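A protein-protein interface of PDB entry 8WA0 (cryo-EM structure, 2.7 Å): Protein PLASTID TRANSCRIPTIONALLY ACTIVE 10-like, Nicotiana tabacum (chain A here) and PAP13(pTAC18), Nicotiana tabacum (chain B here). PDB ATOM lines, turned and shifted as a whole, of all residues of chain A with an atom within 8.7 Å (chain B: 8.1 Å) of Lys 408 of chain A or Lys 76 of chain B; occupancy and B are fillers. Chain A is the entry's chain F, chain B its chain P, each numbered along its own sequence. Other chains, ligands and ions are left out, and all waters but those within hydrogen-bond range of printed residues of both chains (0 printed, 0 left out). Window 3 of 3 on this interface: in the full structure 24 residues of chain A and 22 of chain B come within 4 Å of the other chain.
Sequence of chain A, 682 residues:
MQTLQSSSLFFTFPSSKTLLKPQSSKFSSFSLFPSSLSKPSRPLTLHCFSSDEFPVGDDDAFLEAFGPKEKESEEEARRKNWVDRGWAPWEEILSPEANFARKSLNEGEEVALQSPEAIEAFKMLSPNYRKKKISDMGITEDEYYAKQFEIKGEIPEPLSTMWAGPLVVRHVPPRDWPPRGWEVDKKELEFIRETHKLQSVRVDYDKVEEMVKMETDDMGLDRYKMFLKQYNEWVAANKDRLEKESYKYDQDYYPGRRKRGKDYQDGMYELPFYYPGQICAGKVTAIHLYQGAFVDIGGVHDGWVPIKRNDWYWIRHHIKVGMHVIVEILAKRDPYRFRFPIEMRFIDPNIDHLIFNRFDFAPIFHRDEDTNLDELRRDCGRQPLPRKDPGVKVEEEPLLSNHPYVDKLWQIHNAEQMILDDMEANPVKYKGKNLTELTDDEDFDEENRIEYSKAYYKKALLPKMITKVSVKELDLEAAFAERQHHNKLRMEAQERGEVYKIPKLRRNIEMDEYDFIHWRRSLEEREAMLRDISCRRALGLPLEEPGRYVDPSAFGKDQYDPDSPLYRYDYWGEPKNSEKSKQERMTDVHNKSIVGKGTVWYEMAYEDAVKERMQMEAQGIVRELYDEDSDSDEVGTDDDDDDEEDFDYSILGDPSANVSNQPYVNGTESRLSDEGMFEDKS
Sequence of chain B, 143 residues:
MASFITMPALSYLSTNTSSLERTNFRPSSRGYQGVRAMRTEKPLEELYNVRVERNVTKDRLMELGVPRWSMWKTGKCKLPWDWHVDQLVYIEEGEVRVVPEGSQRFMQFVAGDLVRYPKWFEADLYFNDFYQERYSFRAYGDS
Among the printed residues, merely in contact across the chains: His 403 of chain A with Lys 73 of chain B (3.8 Å), Pro 404 of chain A with Cys 77 of chain B (3.5 Å), Tyr 405 of chain A with Gly 75 of chain B (3.95 Å) and Lys 408 of chain A with Lys 76 of chain B (3.7 Å).
Printed residues of chain A that touch a printed residue of chain B: His 403, Pro 404, Tyr 405 and Lys 408. Along chain A the printed residues that touch a printed residue of chain B span positions 403 to 408. Of the 13 printed residues of chain B, 4 touch a printed residue of chain A. Along chain B the printed residues that touch a printed residue of chain A span positions 73 to 77. Among the printed residues, no Asp or Glu carboxylate lies within 4 Å of a Lys or Arg side-chain nitrogen of the other chain.
Printed residues of chain B within 4 Å of His 403 of chain A: Lys 73. Of the printed residues of chain B, Tyr 405 of chain A touches Gly 75. Lys 408 of chain A touches one residue of chain B. Of the printed residues of chain A, Lys 76 of chain B touches Lys 408 (3.7 Å). The nearest residue of chain B that does not touch Lys 408 of chain A is Cys 77 of chain B (5.5 Å). The nearest residue of chain A that does not touch Lys 76 of chain B is Tyr 405 of chain A (4.2 Å).
The backbone carbonyl oxygen (O) of Gly 75 of chain B is in hydrogen-bond range of the backbone NH (N) of Asp 129 of chain B (3.3 Å). The backbone carbonyl oxygen of Phe 127 of chain B is in hydrogen-bond range of the backbone NH of Cys 77 of chain B, at 2.8 Å. A ring nitrogen (ND1) of His 403 of chain A is in hydrogen-bond range of the backbone NH (N) of Tyr 405 of chain A, at 3.3 Å.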
ATOM      1  N   HIS A 403       5.140   7.140  16.919  1.00  0.00           N
ATOM      2  CA  HIS A 403       4.102   6.389  17.591  1.00  0.00           C
ATOM      3  C   HIS A 403       2.993   7.247  18.236  1.00  0.00           C
ATOM      4  O   HIS A 403       3.298   8.218  18.911  1.00  0.00           O
ATOM      5  CB  HIS A 403       4.696   5.413  18.597  1.00  0.00           C
ATOM      6  CG  HIS A 403       3.820   4.237  18.889  1.00  0.00           C
ATOM      7  ND1 HIS A 403       2.992   4.181  19.989  1.00  0.00           N
ATOM      8  CD2 HIS A 403       3.647   3.070  18.227  1.00  0.00           C
ATOM      9  CE1 HIS A 403       2.345   3.029  19.990  1.00  0.00           C
ATOM     10  NE2 HIS A 403       2.726   2.336  18.933  1.00  0.00           N
ATOM     11  N   PRO A 404       1.695   6.918  18.002  1.00  0.00           N
ATOM     12  CA  PRO A 404       0.647   7.660  18.692  1.00  0.00           C
ATOM     13  C   PRO A 404       0.693   7.683  20.203  1.00  0.00           C
ATOM     14  O   PRO A 404       0.508   8.753  20.772  1.00  0.00           O
ATOM     15  CB  PRO A 404      -0.628   6.935  18.252  1.00  0.00           C
ATOM     16  CG  PRO A 404      -0.293   6.351  16.929  1.00  0.00           C
ATOM     17  CD  PRO A 404       1.146   5.951  17.034  1.00  0.00           C
ATOM     18  N   TYR A 405       0.952   6.558  20.857  1.00  0.00           N
ATOM     19  CA  TYR A 405       0.913   6.515  22.316  1.00  0.00           C
ATOM     20  C   TYR A 405       2.071   7.312  22.878  1.00  0.00           C
ATOM     21  O   TYR A 405       2.089   7.658  24.053  1.00  0.00           O
ATOM     22  CB  TYR A 405       0.916   5.086  22.818  1.00  0.00           C
ATOM     23  CG  TYR A 405       0.940   4.944  24.318  1.00  0.00           C
ATOM     24  CD1 TYR A 405      -0.095   5.435  25.098  1.00  0.00           C
ATOM     25  CD2 TYR A 405       1.999   4.315  24.956  1.00  0.00           C
ATOM     26  CE1 TYR A 405      -0.077   5.309  26.471  1.00  0.00           C
ATOM     27  CE2 TYR A 405       2.027   4.183  26.330  1.00  0.00           C
ATOM     28  CZ  TYR A 405       0.987   4.681  27.083  1.00  0.00           C
ATOM     29  OH  TYR A 405       1.010   4.551  28.452  1.00  0.00           O
ATOM     30  N   VAL A 406       3.032   7.639  22.035  1.00  0.00           N
ATOM     31  CA  VAL A 406       4.198   8.354  22.485  1.00  0.00           C
ATOM     32  C   VAL A 406       3.786   9.659  23.051  1.00  0.00           C
ATOM     33  O   VAL A 406       4.410  10.154  23.978  1.00  0.00           O
ATOM     34  CB  VAL A 406       5.182   8.625  21.344  1.00  0.00           C
ATOM     35  N   ASP A 407       2.764  10.256  22.483  1.00  0.00           N
ATOM     36  CA  ASP A 407       2.410  11.571  22.927  1.00  0.00           C
ATOM     37  C   ASP A 407       2.051  11.535  24.378  1.00  0.00           C
ATOM     38  O   ASP A 407       2.496  12.378  25.154  1.00  0.00           O
ATOM     39  CB  ASP A 407       1.217  12.074  22.133  1.00  0.00           C
ATOM     40  CG  ASP A 407       0.925  13.542  22.380  1.00  0.00           C
ATOM     41  OD1 ASP A 407       1.870  14.297  22.695  1.00  0.00           O
ATOM     42  OD2 ASP A 407      -0.249  13.943  22.247  1.00  0.00           O
ATOM     43  N   LYS A 408       1.286  10.542  24.768  1.00  0.00           N
ATOM     44  CA  LYS A 408       0.869  10.475  26.121  1.00  0.00           C
ATOM     45  C   LYS A 408       2.102  10.304  26.950  1.00  0.00           C
ATOM     46  O   LYS A 408       2.216  10.936  27.969  1.00  0.00           O
ATOM     47  CB  LYS A 408      -0.028   9.276  26.306  1.00  0.00           C
ATOM     48  CG  LYS A 408      -1.073   9.114  25.217  1.00  0.00           C
ATOM     49  CD  LYS A 408      -2.223  10.090  25.396  1.00  0.00           C
ATOM     50  CE  LYS A 408      -3.055   9.736  26.618  1.00  0.00           C
ATOM     51  NZ  LYS A 408      -4.267  10.594  26.731  1.00  0.00           N
ATOM     52  N   LEU A 409       3.042   9.456  26.530  1.00  0.00           N
ATOM     53  CA  LEU A 409       4.227   9.186  27.361  1.00  0.00           C
ATOM     54  C   LEU A 409       5.150  10.357  27.603  1.00  0.00           C
ATOM     55  O   LEU A 409       5.536  10.598  28.714  1.00  0.00           O
ATOM     56  CB  LEU A 409       5.054   8.038  26.784  1.00  0.00           C
ATOM     57  CG  LEU A 409       6.244   7.570  27.626  1.00  0.00           C
ATOM     58  CD1 LEU A 409       5.783   6.821  28.865  1.00  0.00           C
ATOM     59  CD2 LEU A 409       7.158   6.686  26.804  1.00  0.00           C
ATOM     60  N   TRP A 410       5.485  11.105  26.566  1.00  0.00           N
ATOM     61  CA  TRP A 410       6.411  12.195  26.743  1.00  0.00           C
ATOM     62  C   TRP A 410       5.697  13.131  27.649  1.00  0.00           C
ATOM     63  O   TRP A 410       6.295  13.729  28.537  1.00  0.00           O
ATOM     64  CB  TRP A 410       6.810  12.847  25.440  1.00  0.00           C
ATOM     65  CG  TRP A 410       7.662  14.047  25.626  1.00  0.00           C
ATOM     66  CD1 TRP A 410       8.988  14.071  25.928  1.00  0.00           C
ATOM     67  CD2 TRP A 410       7.247  15.411  25.528  1.00  0.00           C
ATOM     68  NE1 TRP A 410       9.429  15.368  26.021  1.00  0.00           N
ATOM     69  CE2 TRP A 410       8.375  16.210  25.778  1.00  0.00           C
ATOM     70  CE3 TRP A 410       6.028  16.035  25.247  1.00  0.00           C
ATOM     71  CZ2 TRP A 410       8.325  17.599  25.758  1.00  0.00           C
ATOM     72  CZ3 TRP A 410       5.980  17.414  25.229  1.00  0.00           C
ATOM     73  CH2 TRP A 410       7.120  18.181  25.483  1.00  0.00           C
ATOM     74  N   GLN A 411       4.413  13.281  27.436  1.00  0.00           N
ATOM     75  CA  GLN A 411       3.660  14.066  28.359  1.00  0.00           C
ATOM     76  C   GLN A 411       3.659  13.394  29.715  1.00  0.00           C
ATOM     77  O   GLN A 411       3.866  14.068  30.707  1.00  0.00           O
ATOM     78  CB  GLN A 411       2.231  14.253  27.855  1.00  0.00           C
ATOM     79  CG  GLN A 411       1.223  14.717  28.897  1.00  0.00           C
ATOM     80  CD  GLN A 411       1.425  16.158  29.331  1.00  0.00           C
ATOM     81  OE1 GLN A 411       2.012  16.964  28.608  1.00  0.00           O
ATOM     82  NE2 GLN A 411       0.925  16.491  30.515  1.00  0.00           N
ATOM     83  N   ILE A 412       3.457  12.085  29.799  1.00  0.00           N
ATOM     84  CA  ILE A 412       3.547  11.444  31.125  1.00  0.00           C
ATOM     85  C   ILE A 412       4.900  11.300  31.855  1.00  0.00           C
ATOM     86  O   ILE A 412       4.936  11.465  33.059  1.00  0.00           O
ATOM     87  CB  ILE A 412       2.690  10.163  31.317  1.00  0.00           C
ATOM     88  CG1 ILE A 412       3.317   8.937  30.659  1.00  0.00           C
ATOM     89  CG2 ILE A 412       1.246  10.395  30.891  1.00  0.00           C
ATOM     90  CD1 ILE A 412       2.477   7.685  30.788  1.00  0.00           C
ATOM     91  N   HIS A 413       5.994  10.965  31.170  1.00  0.00           N
ATOM     92  CA  HIS A 413       7.260  10.750  31.881  1.00  0.00           C
ATOM     93  C   HIS A 413       7.671  12.046  32.512  1.00  0.00           C
ATOM     94  O   HIS A 413       8.044  12.079  33.677  1.00  0.00           O
ATOM     95  CB  HIS A 413       8.347  10.131  30.987  1.00  0.00           C
ATOM     96  N   ASN A 414       7.533  13.131  31.775  1.00  0.00           N
ATOM     97  CA  ASN A 414       7.814  14.412  32.351  1.00  0.00           C
ATOM     98  C   ASN A 414       6.832  14.682  33.456  1.00  0.00           C
ATOM     99  O   ASN A 414       7.204  15.212  34.486  1.00  0.00           O
ATOM    100  CB  ASN A 414       7.713  15.502  31.289  1.00  0.00           C
ATOM    101  CG  ASN A 414       8.916  15.532  30.369  1.00  0.00           C
ATOM    102  OD1 ASN A 414      10.006  15.101  30.742  1.00  0.00           O
ATOM    103  ND2 ASN A 414       8.728  16.058  29.166  1.00  0.00           N
ATOM    104  N   ALA A 415       5.558  14.372  33.245  1.00  0.00           N
ATOM    105  CA  ALA A 415       4.550  14.718  34.253  1.00  0.00           C
ATOM    106  C   ALA A 415       4.843  14.047  35.571  1.00  0.00           C
ATOM    107  O   ALA A 415       4.795  14.680  36.627  1.00  0.00           O
ATOM    108  CB  ALA A 415       3.153  14.357  33.782  1.00  0.00           C
ATOM    109  N   GLU A 416       5.157  12.762  35.515  1.00  0.00           N
ATOM    110  CA  GLU A 416       5.447  12.037  36.731  1.00  0.00           C
ATOM    111  C   GLU A 416       6.660  12.654  37.383  1.00  0.00           C
ATOM    112  O   GLU A 416       6.662  12.918  38.582  1.00  0.00           O
ATOM    113  CB  GLU A 416       5.752  10.576  36.406  1.00  0.00           C
ATOM    114  CG  GLU A 416       4.580   9.802  35.838  1.00  0.00           C
ATOM    115  CD  GLU A 416       4.976   8.420  35.370  1.00  0.00           C
ATOM    116  OE1 GLU A 416       6.181   8.098  35.421  1.00  0.00           O
ATOM    117  OE2 GLU A 416       4.082   7.658  34.952  1.00  0.00           O
ATOM    118  N   GLU A 446      -9.511  16.288  33.593  1.00  0.00           N
ATOM    119  CA  GLU A 446      -8.652  16.463  32.427  1.00  0.00           C
ATOM    120  C   GLU A 446      -9.421  17.093  31.273  1.00  0.00           C
ATOM    121  O   GLU A 446      -8.907  17.980  30.582  1.00  0.00           O
ATOM    122  CB  GLU A 446      -8.045  15.125  32.009  1.00  0.00           C
ATOM    123  N   LYS A 468      -4.344  18.480  31.827  1.00  0.00           N
ATOM    124  CA  LYS A 468      -4.380  17.989  33.197  1.00  0.00           C
ATOM    125  C   LYS A 468      -3.905  16.555  33.270  1.00  0.00           C
ATOM    126  O   LYS A 468      -4.413  15.687  32.561  1.00  0.00           O
ATOM    127  CB  LYS A 468      -5.786  18.095  33.788  1.00  0.00           C
ATOM    128  N   VAL A 469      -2.934  16.297  34.135  1.00  0.00           N
ATOM    129  CA  VAL A 469      -2.471  14.940  34.300  1.00  0.00           C
ATOM    130  C   VAL A 469      -3.175  14.395  35.512  1.00  0.00           C
ATOM    131  O   VAL A 469      -3.027  14.920  36.611  1.00  0.00           O
ATOM    132  CB  VAL A 469      -0.960  14.890  34.551  1.00  0.00           C
ATOM    133  N   GLU A 473      -3.284   8.694  37.399  1.00  0.00           N
ATOM    134  CA  GLU A 473      -2.531   8.171  36.276  1.00  0.00           C
ATOM    135  C   GLU A 473      -1.032   8.154  36.549  1.00  0.00           C
ATOM    136  O   GLU A 473      -0.351   7.190  36.197  1.00  0.00           O
ATOM    137  CB  GLU A 473      -2.874   8.957  35.000  1.00  0.00           C
ATOM    138  N   LEU A 474      -0.509   9.190  37.192  1.00  0.00           N
ATOM    139  CA  LEU A 474       0.933   9.263  37.375  1.00  0.00           C
ATOM    140  C   LEU A 474       1.476   8.151  38.253  1.00  0.00           C
ATOM    141  O   LEU A 474       0.920   7.868  39.314  1.00  0.00           O
ATOM    142  CB  LEU A 474       1.318  10.623  37.942  1.00  0.00           C
ATOM    143  CG  LEU A 474       0.858  11.823  37.116  1.00  0.00           C
ATOM    144  CD1 LEU A 474       1.311  13.122  37.757  1.00  0.00           C
ATOM    145  CD2 LEU A 474       1.366  11.722  35.687  1.00  0.00           C
ATOM    146  N   MET A 511      10.027   4.789  25.419  1.00  0.00           N
ATOM    147  CA  MET A 511       9.577   5.540  24.303  1.00  0.00           C
ATOM    148  C   MET A 511      10.061   4.844  23.081  1.00  0.00           C
ATOM    149  O   MET A 511       9.289   4.620  22.153  1.00  0.00           O
ATOM    150  CB  MET A 511      10.173   6.931  24.350  1.00  0.00           C
ATOM    151  CG  MET A 511       9.219   8.034  23.935  1.00  0.00           C
ATOM    152  SD  MET A 511       9.782   9.661  24.467  1.00  0.00           S
ATOM    153  CE  MET A 511       9.860   9.443  26.243  1.00  0.00           C
ATOM    154  N   TYR A 514       7.867   1.374  22.660  1.00  0.00           N
ATOM    155  CA  TYR A 514       6.540   1.487  22.075  1.00  0.00           C
ATOM    156  C   TYR A 514       6.765   1.861  20.654  1.00  0.00           C
ATOM    157  O   TYR A 514       6.074   1.406  19.764  1.00  0.00           O
ATOM    158  CB  TYR A 514       5.695   2.540  22.759  1.00  0.00           C
ATOM    159  CG  TYR A 514       5.639   2.413  24.258  1.00  0.00           C
ATOM    160  CD1 TYR A 514       5.524   1.172  24.866  1.00  0.00           C
ATOM    161  CD2 TYR A 514       5.688   3.537  25.068  1.00  0.00           C
ATOM    162  CE1 TYR A 514       5.478   1.055  26.241  1.00  0.00           C
ATOM    163  CE2 TYR A 514       5.635   3.429  26.442  1.00  0.00           C
ATOM    164  CZ  TYR A 514       5.528   2.186  27.023  1.00  0.00           C
ATOM    165  OH  TYR A 514       5.474   2.076  28.394  1.00  0.00           O
ATOM    166  N   LYS B  73       1.017  -2.866  20.405  1.00  0.00           N
ATOM    167  CA  LYS B  73       0.410  -2.559  21.690  1.00  0.00           C
ATOM    168  C   LYS B  73       0.182  -1.063  21.884  1.00  0.00           C
ATOM    169  O   LYS B  73       0.973  -0.260  21.393  1.00  0.00           O
ATOM    170  CB  LYS B  73       1.288  -3.146  22.806  1.00  0.00           C
ATOM    171  N   THR B  74      -0.890  -0.684  22.590  1.00  0.00           N
ATOM    172  CA  THR B  74      -1.170   0.710  22.805  1.00  0.00           C
ATOM    173  C   THR B  74      -2.020   0.879  24.004  1.00  0.00           C
ATOM    174  O   THR B  74      -2.565  -0.079  24.520  1.00  0.00           O
ATOM    175  CB  THR B  74      -1.941   1.358  21.642  1.00  0.00           C
ATOM    176  N   GLY B  75      -2.131   2.105  24.471  1.00  0.00           N
ATOM    177  CA  GLY B  75      -3.020   2.369  25.573  1.00  0.00           C
ATOM    178  C   GLY B  75      -4.148   3.204  25.055  1.00  0.00           C
ATOM    179  O   GLY B  75      -4.952   2.738  24.257  1.00  0.00           O
ATOM    180  N   LYS B  76      -4.201   4.462  25.451  1.00  0.00           N
ATOM    181  CA  LYS B  76      -5.217   5.332  24.909  1.00  0.00           C
ATOM    182  C   LYS B  76      -4.655   6.151  23.751  1.00  0.00           C
ATOM    183  O   LYS B  76      -3.834   7.044  23.973  1.00  0.00           O
ATOM    184  CB  LYS B  76      -5.708   6.273  25.992  1.00  0.00           C
ATOM    185  N   CYS B  77      -5.091   5.864  22.521  1.00  0.00           N
ATOM    186  CA  CYS B  77      -4.642   6.636  21.354  1.00  0.00           C
ATOM    187  C   CYS B  77      -5.557   6.529  20.120  1.00  0.00           C
ATOM    188  O   CYS B  77      -6.392   5.629  20.055  1.00  0.00           O
ATOM    189  CB  CYS B  77      -3.198   6.274  20.993  1.00  0.00           C
ATOM    190  SG  CYS B  77      -3.063   4.981  19.747  1.00  0.00           S
ATOM    191  N   LYS B  78      -5.420   7.443  19.154  1.00  0.00           N
ATOM    192  CA  LYS B  78      -6.202   7.391  17.908  1.00  0.00           C
ATOM    193  C   LYS B  78      -5.257   7.387  16.743  1.00  0.00           C
ATOM    194  O   LYS B  78      -4.318   8.169  16.715  1.00  0.00           O
ATOM    195  CB  LYS B  78      -7.097   8.599  17.802  1.00  0.00           C
ATOM    196  N   LEU B  79      -5.465   6.505  15.784  1.00  0.00           N
ATOM    197  CA  LEU B  79      -4.569   6.398  14.655  1.00  0.00           C
ATOM    198  C   LEU B  79      -5.276   6.514  13.344  1.00  0.00           C
ATOM    199  O   LEU B  79      -6.239   5.819  13.083  1.00  0.00           O
ATOM    200  CB  LEU B  79      -3.914   5.023  14.679  1.00  0.00           C
ATOM    201  N   TYR B 126      -9.614   4.132  16.832  1.00  0.00           N
ATOM    202  CA  TYR B 126      -9.555   4.744  18.144  1.00  0.00           C
ATOM    203  C   TYR B 126      -9.637   3.736  19.283  1.00  0.00           C
ATOM    204  O   TYR B 126     -10.604   2.985  19.350  1.00  0.00           O
ATOM    205  CB  TYR B 126     -10.711   5.688  18.339  1.00  0.00           C
ATOM    206  CG  TYR B 126     -10.768   6.989  17.575  1.00  0.00           C
ATOM    207  CD1 TYR B 126     -10.834   7.016  16.195  1.00  0.00           C
ATOM    208  CD2 TYR B 126     -10.856   8.193  18.254  1.00  0.00           C
ATOM    209  CE1 TYR B 126     -10.929   8.211  15.513  1.00  0.00           C
ATOM    210  CE2 TYR B 126     -10.957   9.389  17.581  1.00  0.00           C
ATOM    211  CZ  TYR B 126     -10.991   9.394  16.212  1.00  0.00           C
ATOM    212  OH  TYR B 126     -11.082  10.587  15.532  1.00  0.00           O
ATOM    213  N   PHE B 127      -8.649   3.737  20.196  1.00  0.00           N
ATOM    214  CA  PHE B 127      -8.634   2.833  21.372  1.00  0.00           C
ATOM    215  C   PHE B 127      -8.386   3.587  22.670  1.00  0.00           C
ATOM    216  O   PHE B 127      -7.518   4.443  22.702  1.00  0.00           O
ATOM    217  CB  PHE B 127      -7.565   1.745  21.261  1.00  0.00           C
ATOM    218  N   ASN B 128      -9.129   3.295  23.734  1.00  0.00           N
ATOM    219  CA  ASN B 128      -8.889   3.929  25.039  1.00  0.00           C
ATOM    220  C   ASN B 128      -8.134   3.128  26.101  1.00  0.00           C
ATOM    221  O   ASN B 128      -7.935   3.641  27.197  1.00  0.00           O
ATOM    222  CB  ASN B 128     -10.194   4.353  25.666  1.00  0.00           C
ATOM    223  CG  ASN B 128     -11.121   3.184  25.947  1.00  0.00           C
ATOM    224  OD1 ASN B 128     -10.973   2.099  25.386  1.00  0.00           O
ATOM    225  ND2 ASN B 128     -12.097   3.409  26.817  1.00  0.00           N
ATOM    226  N   ASP B 129      -7.772   1.873  25.833  1.00  0.00           N
ATOM    227  CA  ASP B 129      -7.132   1.018  26.853  1.00  0.00           C
ATOM    228  C   ASP B 129      -6.039   0.112  26.312  1.00  0.00           C
ATOM    229  O   ASP B 129      -5.583   0.280  25.190  1.00  0.00           O
ATOM    230  CB  ASP B 129      -8.171   0.138  27.547  1.00  0.00           C
ATOM    231  CG  ASP B 129      -9.037   0.905  28.516  1.00  0.00           C
ATOM    232  OD1 ASP B 129      -8.481   1.653  29.347  1.00  0.00           O
ATOM    233  OD2 ASP B 129     -10.274   0.752  28.454  1.00  0.00           O
ATOM    234  N   PHE B 130      -5.662  -0.902  27.080  1.00  0.00           N
ATOM    235  CA  PHE B 130      -4.559  -1.756  26.663  1.00  0.00           C
ATOM    236  C   PHE B 130      -4.832  -2.470  25.357  1.00  0.00           C
ATOM    237  O   PHE B 130      -5.948  -2.921  25.106  1.00  0.00           O
ATOM    238  CB  PHE B 130      -4.205  -2.770  27.748  1.00  0.00           C
ATOM    239  CG  PHE B 130      -3.026  -3.635  27.398  1.00  0.00           C
ATOM    240  CD1 PHE B 130      -1.744  -3.107  27.386  1.00  0.00           C
ATOM    241  CD2 PHE B 130      -3.197  -4.968  27.062  1.00  0.00           C
ATOM    242  CE1 PHE B 130      -0.659  -3.894  27.055  1.00  0.00           C
ATOM    243  CE2 PHE B 130      -2.113  -5.759  26.729  1.00  0.00           C
ATOM    244  CZ  PHE B 130      -0.842  -5.222  26.726  1.00  0.00           C
ATOM    245  N   TYR B 131      -3.805  -2.576  24.525  1.00  0.00           N
ATOM    246  CA  TYR B 131      -3.977  -3.186  23.229  1.00  0.00           C
ATOM    247  C   TYR B 131      -2.954  -4.253  22.973  1.00  0.00           C
ATOM    248  O   TYR B 131      -1.807  -4.109  23.356  1.00  0.00           O
ATOM    249  CB  TYR B 131      -3.852  -2.099  22.173  1.00  0.00           C
ATOM    250  CG  TYR B 131      -4.439  -2.421  20.826  1.00  0.00           C
ATOM    251  CD1 TYR B 131      -5.790  -2.240  20.580  1.00  0.00           C
ATOM    252  CD2 TYR B 131      -3.638  -2.866  19.788  1.00  0.00           C
ATOM    253  CE1 TYR B 131      -6.336  -2.529  19.348  1.00  0.00           C
ATOM    254  CE2 TYR B 131      -4.174  -3.151  18.551  1.00  0.00           C
ATOM    255  CZ  TYR B 131      -5.524  -2.983  18.337  1.00  0.00           C
ATOM    256  OH  TYR B 131      -6.061  -3.267  17.105  1.00  0.00           O
